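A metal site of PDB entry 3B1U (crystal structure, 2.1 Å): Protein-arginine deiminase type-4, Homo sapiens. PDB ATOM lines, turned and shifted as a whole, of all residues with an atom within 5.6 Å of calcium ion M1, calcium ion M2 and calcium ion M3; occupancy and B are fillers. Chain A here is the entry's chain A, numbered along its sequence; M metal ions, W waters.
O of Asn 161 is in hydrogen-bond range of SG of Cys 174 (3.3 Å). The side-chain carboxylate (OE1) of Glu 260 sits at hydrogen-bond distance from the side-chain amide nitrogen (ND2) of Asn 161, at 2.7 Å.
Six residues have an atom within 4 Å of calcium ion M2: Asn 161, Asp 163, Asp 165, Asp 173, Asp 184 and Asp 187. The nearest printed residue that does not touch calcium ion M2 is Arg 164 (5.1 Å).
Along chain A the residues within 4 Å of calcium ion M3 span positions 163 to 396.
Calcium ion M1 is bound by the backbone carbonyl oxygen (O) of Glu 178 (2.3 Å). Water W3 binds calcium ion M1, at 2.3 Å. O of Asp 173 binds calcium ion M1 (2.3 Å). Calcium ion M1 is bound by the side-chain carboxylate (OD2) of Asp 176 (2.4 Å). Water W1 binds calcium ion M1 (2.4 Å).
Calcium ion M2 is bound by OD2 of Asp 187 (2.3 Å). Calcium ion M2 is bound by the side-chain carboxylate (OD2) of Asp 184 (2.3 Å). OD1 of Asp 163 binds calcium ion M2 (2.4 Å). Calcium ion M2 is bound by OD1 of Asn 161, at 2.4 Å. OD2 of Asp 165 is bound to calcium ion M2. The side-chain carboxylate (OD2) of Asp 173 is bound to calcium ion M2 (2.5 Å).
Calcium ion M3 is bound by the side-chain carboxylate (OD1) of Asp 396, at 2.2 Å. Water W2 binds calcium ion M3. Calcium ion M3 is bound by OD2 of Asp 163 (2.4 Å). OD2 of Asp 187 is bound to calcium ion M3 (2.5 Å). OD1 of Asp 165 binds calcium ion M3 (2.6 Å). OD2 of Asp 165 is bound to calcium ion M3 (2.6 Å). Calcium ion M3 is bound by OD1 of Asp 187 (2.9 Å). Calcium ion M3 has seven donor atoms within binding distance.
Water W3 lies within hydrogen-bond range of the side-chain carboxylate of Asp 184 (2.7 Å), the side-chain carboxylate of Glu 260 (2.7 Å) and the side-chain amide nitrogen of Asn 161 (3.1 Å). Water W1 lies within hydrogen-bond range of the backbone carbonyl oxygen (O) of Asp 176 (2.7 Å) and the side-chain carboxylate (OE2) of Glu 260 (2.7 Å).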
ATOM      1  N   ASN A 161      11.261  23.272  -9.683  1.00  0.00           N
ATOM      2  CA  ASN A 161      12.052  22.529 -10.667  1.00  0.00           C
ATOM      3  C   ASN A 161      13.504  22.411 -10.190  1.00  0.00           C
ATOM      4  O   ASN A 161      14.431  22.973 -10.782  1.00  0.00           O
ATOM      5  CB  ASN A 161      11.963  23.216 -12.033  1.00  0.00           C
ATOM      6  CG  ASN A 161      12.436  22.334 -13.178  1.00  0.00           C
ATOM      7  OD1 ASN A 161      12.757  21.155 -13.001  1.00  0.00           O
ATOM      8  ND2 ASN A 161      12.490  22.908 -14.376  1.00  0.00           N
ATOM      9  N   ASP A 163      15.401  19.568  -9.701  1.00  0.00           N
ATOM     10  CA  ASP A 163      16.208  18.448 -10.173  1.00  0.00           C
ATOM     11  C   ASP A 163      17.080  18.898 -11.337  1.00  0.00           C
ATOM     12  O   ASP A 163      17.121  20.080 -11.665  1.00  0.00           O
ATOM     13  CB  ASP A 163      15.315  17.247 -10.537  1.00  0.00           C
ATOM     14  CG  ASP A 163      14.551  17.454 -11.841  1.00  0.00           C
ATOM     15  OD1 ASP A 163      14.287  18.609 -12.214  1.00  0.00           O
ATOM     16  OD2 ASP A 163      14.196  16.437 -12.478  1.00  0.00           O
ATOM     17  N   ARG A 164      17.798  17.957 -11.949  1.00  0.00           N
ATOM     18  CA  ARG A 164      18.709  18.269 -13.043  1.00  0.00           C
ATOM     19  C   ARG A 164      18.597  17.262 -14.191  1.00  0.00           C
ATOM     20  O   ARG A 164      19.342  16.283 -14.255  1.00  0.00           O
ATOM     21  CB  ARG A 164      20.151  18.314 -12.524  1.00  0.00           C
ATOM     22  CG  ARG A 164      21.158  18.881 -13.497  1.00  0.00           C
ATOM     23  CD  ARG A 164      22.542  18.869 -12.880  1.00  0.00           C
ATOM     24  NE  ARG A 164      23.107  17.520 -12.869  1.00  0.00           N
ATOM     25  CZ  ARG A 164      23.871  17.005 -11.915  1.00  0.00           C
ATOM     26  NH1 ARG A 164      24.187  17.700 -10.817  1.00  0.00           N
ATOM     27  NH2 ARG A 164      24.314  15.760 -12.037  1.00  0.00           N
ATOM     28  N   ASP A 165      17.642  17.504 -15.085  1.00  0.00           N
ATOM     29  CA  ASP A 165      17.434  16.654 -16.265  1.00  0.00           C
ATOM     30  C   ASP A 165      18.501  16.899 -17.324  1.00  0.00           C
ATOM     31  O   ASP A 165      18.814  16.010 -18.119  1.00  0.00           O
ATOM     32  CB  ASP A 165      16.054  16.894 -16.865  1.00  0.00           C
ATOM     33  CG  ASP A 165      14.946  16.495 -15.928  1.00  0.00           C
ATOM     34  OD1 ASP A 165      14.907  15.322 -15.498  1.00  0.00           O
ATOM     35  OD2 ASP A 165      14.086  17.348 -15.618  1.00  0.00           O
ATOM     36  N   ASP A 173      17.821  22.885 -12.890  1.00  0.00           N
ATOM     37  CA  ASP A 173      17.193  23.334 -14.136  1.00  0.00           C
ATOM     38  C   ASP A 173      16.581  24.735 -14.024  1.00  0.00           C
ATOM     39  O   ASP A 173      16.542  25.468 -15.019  1.00  0.00           O
ATOM     40  CB  ASP A 173      16.121  22.335 -14.589  1.00  0.00           C
ATOM     41  CG  ASP A 173      16.693  20.965 -14.934  1.00  0.00           C
ATOM     42  OD1 ASP A 173      17.864  20.876 -15.360  1.00  0.00           O
ATOM     43  OD2 ASP A 173      15.949  19.959 -14.804  1.00  0.00           O
ATOM     44  N   CYS A 174      16.096  25.100 -12.835  1.00  0.00           N
ATOM     45  CA  CYS A 174      15.408  26.381 -12.630  1.00  0.00           C
ATOM     46  C   CYS A 174      16.335  27.599 -12.417  1.00  0.00           C
ATOM     47  O   CYS A 174      15.854  28.717 -12.253  1.00  0.00           O
ATOM     48  CB  CYS A 174      14.442  26.277 -11.451  1.00  0.00           C
ATOM     49  SG  CYS A 174      15.218  26.029  -9.842  1.00  0.00           S
ATOM     50  N   GLU A 175      17.646  27.373 -12.415  1.00  0.00           N
ATOM     51  CA  GLU A 175      18.612  28.457 -12.186  1.00  0.00           C
ATOM     52  C   GLU A 175      18.839  29.355 -13.419  1.00  0.00           C
ATOM     53  O   GLU A 175      19.311  30.479 -13.271  1.00  0.00           O
ATOM     54  CB  GLU A 175      19.950  27.889 -11.708  1.00  0.00           C
ATOM     55  CG  GLU A 175      19.895  27.325 -10.294  1.00  0.00           C
ATOM     56  CD  GLU A 175      21.242  26.785  -9.819  1.00  0.00           C
ATOM     57  OE1 GLU A 175      22.269  27.453 -10.057  1.00  0.00           O
ATOM     58  OE2 GLU A 175      21.262  25.701  -9.195  1.00  0.00           O
ATOM     59  N   ASP A 176      18.509  28.857 -14.616  1.00  0.00           N
ATOM     60  CA  ASP A 176      18.590  29.662 -15.836  1.00  0.00           C
ATOM     61  C   ASP A 176      17.182  29.998 -16.346  1.00  0.00           C
ATOM     62  O   ASP A 176      16.195  29.611 -15.724  1.00  0.00           O
ATOM     63  CB  ASP A 176      19.413  28.934 -16.926  1.00  0.00           C
ATOM     64  CG  ASP A 176      18.727  27.696 -17.471  1.00  0.00           C
ATOM     65  OD1 ASP A 176      19.328  27.029 -18.343  1.00  0.00           O
ATOM     66  OD2 ASP A 176      17.594  27.367 -17.048  1.00  0.00           O
ATOM     67  N   ASP A 177      17.099  30.715 -17.457  1.00  0.00           N
ATOM     68  CA  ASP A 177      15.804  31.094 -18.043  1.00  0.00           C
ATOM     69  C   ASP A 177      15.608  30.469 -19.432  1.00  0.00           C
ATOM     70  O   ASP A 177      15.192  31.151 -20.381  1.00  0.00           O
ATOM     71  CB  ASP A 177      15.616  32.613 -18.057  1.00  0.00           C
ATOM     72  CG  ASP A 177      16.865  33.360 -18.483  1.00  0.00           C
ATOM     73  OD1 ASP A 177      17.200  33.334 -19.686  1.00  0.00           O
ATOM     74  OD2 ASP A 177      17.506  33.986 -17.607  1.00  0.00           O
ATOM     75  N   GLU A 178      15.879  29.174 -19.529  1.00  0.00           N
ATOM     76  CA  GLU A 178      15.678  28.394 -20.751  1.00  0.00           C
ATOM     77  C   GLU A 178      15.212  26.978 -20.419  1.00  0.00           C
ATOM     78  O   GLU A 178      15.562  26.435 -19.374  1.00  0.00           O
ATOM     79  CB  GLU A 178      16.974  28.306 -21.564  1.00  0.00           C
ATOM     80  CG  GLU A 178      17.618  29.634 -21.920  1.00  0.00           C
ATOM     81  CD  GLU A 178      18.821  29.469 -22.832  1.00  0.00           C
ATOM     82  OE1 GLU A 178      18.706  28.791 -23.866  1.00  0.00           O
ATOM     83  OE2 GLU A 178      19.893  30.040 -22.508  1.00  0.00           O
ATOM     84  N   VAL A 179      14.430  26.386 -21.326  1.00  0.00           N
ATOM     85  CA  VAL A 179      14.093  24.961 -21.240  1.00  0.00           C
ATOM     86  C   VAL A 179      15.076  24.192 -22.129  1.00  0.00           C
ATOM     87  O   VAL A 179      14.920  24.150 -23.345  1.00  0.00           O
ATOM     88  CB  VAL A 179      12.649  24.687 -21.700  1.00  0.00           C
ATOM     89  CG1 VAL A 179      12.336  23.199 -21.634  1.00  0.00           C
ATOM     90  CG2 VAL A 179      11.660  25.477 -20.857  1.00  0.00           C
ATOM     91  N   LEU A 180      16.081  23.584 -21.501  1.00  0.00           N
ATOM     92  CA  LEU A 180      17.181  22.939 -22.225  1.00  0.00           C
ATOM     93  C   LEU A 180      16.829  21.545 -22.759  1.00  0.00           C
ATOM     94  O   LEU A 180      17.342  21.142 -23.804  1.00  0.00           O
ATOM     95  CB  LEU A 180      18.435  22.861 -21.355  1.00  0.00           C
ATOM     96  CG  LEU A 180      19.115  24.203 -21.048  1.00  0.00           C
ATOM     97  CD1 LEU A 180      20.201  24.022 -19.995  1.00  0.00           C
ATOM     98  CD2 LEU A 180      19.688  24.821 -22.319  1.00  0.00           C
ATOM     99  N   GLU A 183      12.458  16.622 -21.707  1.00  0.00           N
ATOM    100  CA  GLU A 183      12.066  15.896 -20.490  1.00  0.00           C
ATOM    101  C   GLU A 183      11.801  16.841 -19.322  1.00  0.00           C
ATOM    102  O   GLU A 183      10.992  16.543 -18.444  1.00  0.00           O
ATOM    103  CB  GLU A 183      13.138  14.872 -20.086  1.00  0.00           C
ATOM    104  CG  GLU A 183      13.331  13.711 -21.056  1.00  0.00           C
ATOM    105  CD  GLU A 183      14.279  14.018 -22.209  1.00  0.00           C
ATOM    106  OE1 GLU A 183      14.385  13.176 -23.131  1.00  0.00           O
ATOM    107  OE2 GLU A 183      14.918  15.085 -22.205  1.00  0.00           O
ATOM    108  N   ASP A 184      12.501  17.973 -19.312  1.00  0.00           N
ATOM    109  CA  ASP A 184      12.352  19.004 -18.283  1.00  0.00           C
ATOM    110  C   ASP A 184      10.905  19.530 -18.184  1.00  0.00           C
ATOM    111  O   ASP A 184      10.446  19.875 -17.100  1.00  0.00           O
ATOM    112  CB  ASP A 184      13.314  20.167 -18.549  1.00  0.00           C
ATOM    113  CG  ASP A 184      13.351  21.189 -17.416  1.00  0.00           C
ATOM    114  OD1 ASP A 184      13.385  22.398 -17.708  1.00  0.00           O
ATOM    115  OD2 ASP A 184      13.349  20.770 -16.233  1.00  0.00           O
ATOM    116  N   ASP A 187       8.308  18.157 -15.578  1.00  0.00           N
ATOM    117  CA  ASP A 187       8.293  18.698 -14.218  1.00  0.00           C
ATOM    118  C   ASP A 187       7.448  19.958 -14.082  1.00  0.00           C
ATOM    119  O   ASP A 187       7.115  20.354 -12.964  1.00  0.00           O
ATOM    120  CB  ASP A 187       9.715  19.016 -13.768  1.00  0.00           C
ATOM    121  CG  ASP A 187      10.597  17.797 -13.698  1.00  0.00           C
ATOM    122  OD1 ASP A 187      10.096  16.686 -13.441  1.00  0.00           O
ATOM    123  OD2 ASP A 187      11.818  17.951 -13.915  1.00  0.00           O
ATOM    124  N   MET A 188       7.106  20.585 -15.198  1.00  0.00           N
ATOM    125  CA  MET A 188       6.404  21.874 -15.187  1.00  0.00           C
ATOM    126  C   MET A 188       4.900  21.701 -15.277  1.00  0.00           C
ATOM    127  O   MET A 188       4.410  20.673 -15.751  1.00  0.00           O
ATOM    128  CB  MET A 188       6.910  22.740 -16.344  1.00  0.00           C
ATOM    129  CG  MET A 188       8.409  22.983 -16.304  1.00  0.00           C
ATOM    130  SD  MET A 188       8.944  24.232 -17.482  1.00  0.00           S
ATOM    131  CE  MET A 188      10.713  23.978 -17.449  1.00  0.00           C
ATOM    132  N   PHE A 222       7.193  29.760 -19.397  1.00  0.00           N
ATOM    133  CA  PHE A 222       7.653  29.633 -20.779  1.00  0.00           C
ATOM    134  C   PHE A 222       6.459  29.520 -21.718  1.00  0.00           C
ATOM    135  O   PHE A 222       5.453  28.897 -21.368  1.00  0.00           O
ATOM    136  CB  PHE A 222       8.528  28.390 -20.951  1.00  0.00           C
ATOM    137  CG  PHE A 222       9.774  28.402 -20.101  1.00  0.00           C
ATOM    138  CD1 PHE A 222       9.756  27.851 -18.828  1.00  0.00           C
ATOM    139  CD2 PHE A 222      10.954  28.960 -20.576  1.00  0.00           C
ATOM    140  CE1 PHE A 222      10.897  27.853 -18.037  1.00  0.00           C
ATOM    141  CE2 PHE A 222      12.091  28.966 -19.793  1.00  0.00           C
ATOM    142  CZ  PHE A 222      12.071  28.419 -18.529  1.00  0.00           C
ATOM    143  N   GLU A 260       7.206  26.776 -13.969  1.00  0.00           N
ATOM    144  CA  GLU A 260       8.059  26.155 -12.950  1.00  0.00           C
ATOM    145  C   GLU A 260       8.179  27.065 -11.741  1.00  0.00           C
ATOM    146  O   GLU A 260       8.206  28.294 -11.890  1.00  0.00           O
ATOM    147  CB  GLU A 260       9.454  25.853 -13.517  1.00  0.00           C
ATOM    148  CG  GLU A 260      10.205  27.078 -14.038  1.00  0.00           C
ATOM    149  CD  GLU A 260      11.614  26.774 -14.521  1.00  0.00           C
ATOM    150  OE1 GLU A 260      11.938  25.578 -14.709  1.00  0.00           O
ATOM    151  OE2 GLU A 260      12.394  27.727 -14.706  1.00  0.00           O
ATOM    152  N   LYS A 370       3.399  14.894 -11.893  1.00  0.00           N
ATOM    153  CA  LYS A 370       4.779  14.470 -11.653  1.00  0.00           C
ATOM    154  C   LYS A 370       5.113  14.357 -10.162  1.00  0.00           C
ATOM    155  O   LYS A 370       4.752  15.211  -9.353  1.00  0.00           O
ATOM    156  CB  LYS A 370       5.742  15.450 -12.333  1.00  0.00           C
ATOM    157  CG  LYS A 370       7.228  15.185 -12.102  1.00  0.00           C
ATOM    158  CD  LYS A 370       7.707  13.888 -12.758  1.00  0.00           C
ATOM    159  CE  LYS A 370       7.862  14.039 -14.259  1.00  0.00           C
ATOM    160  NZ  LYS A 370       8.462  12.830 -14.888  1.00  0.00           N
ATOM    161  N   LEU A 372       8.683  13.320  -7.838  1.00  0.00           N
ATOM    162  CA  LEU A 372      10.108  12.983  -7.836  1.00  0.00           C
ATOM    163  C   LEU A 372      10.728  13.090  -6.445  1.00  0.00           C
ATOM    164  O   LEU A 372      10.294  13.907  -5.638  1.00  0.00           O
ATOM    165  CB  LEU A 372      10.884  13.879  -8.812  1.00  0.00           C
ATOM    166  CG  LEU A 372      10.782  15.396  -8.642  1.00  0.00           C
ATOM    167  CD1 LEU A 372      12.073  16.093  -9.079  1.00  0.00           C
ATOM    168  CD2 LEU A 372       9.591  15.949  -9.410  1.00  0.00           C
ATOM    169  N   PRO A 395      18.842  13.616 -12.786  1.00  0.00           N
ATOM    170  CA  PRO A 395      17.580  13.410 -13.514  1.00  0.00           C
ATOM    171  C   PRO A 395      16.474  12.831 -12.635  1.00  0.00           C
ATOM    172  O   PRO A 395      16.610  11.722 -12.114  1.00  0.00           O
ATOM    173  CB  PRO A 395      17.986  12.416 -14.624  1.00  0.00           C
ATOM    174  CG  PRO A 395      19.433  12.659 -14.836  1.00  0.00           C
ATOM    175  CD  PRO A 395      19.984  13.009 -13.486  1.00  0.00           C
ATOM    176  N   ASP A 396      15.396  13.598 -12.475  1.00  0.00           N
ATOM    177  CA  ASP A 396      14.276  13.232 -11.590  1.00  0.00           C
ATOM    178  C   ASP A 396      14.712  12.997 -10.133  1.00  0.00           C
ATOM    179  O   ASP A 396      14.126  12.173  -9.427  1.00  0.00           O
ATOM    180  CB  ASP A 396      13.506  12.011 -12.135  1.00  0.00           C
ATOM    181  CG  ASP A 396      12.778  12.313 -13.437  1.00  0.00           C
ATOM    182  OD1 ASP A 396      12.407  13.488 -13.667  1.00  0.00           O
ATOM    183  OD2 ASP A 396      12.575  11.387 -14.246  1.00  0.00           O
HETATM  184 CA    CA M   1      15.857  25.692 -17.226  1.00  0.00          CA
HETATM  185 CA    CA M   2      13.594  19.372 -14.382  1.00  0.00          CA
HETATM  186 CA    CA M   3      12.658  15.660 -14.192  1.00  0.00          CA
HETATM  187  O   HOH W   1      14.602  27.559 -16.292  1.00  0.00           O
HETATM  188  O   HOH W   2      11.999  15.145 -16.305  1.00  0.00           O
HETATM  189  O   HOH W   3      13.865  24.789 -16.494  1.00  0.00           O
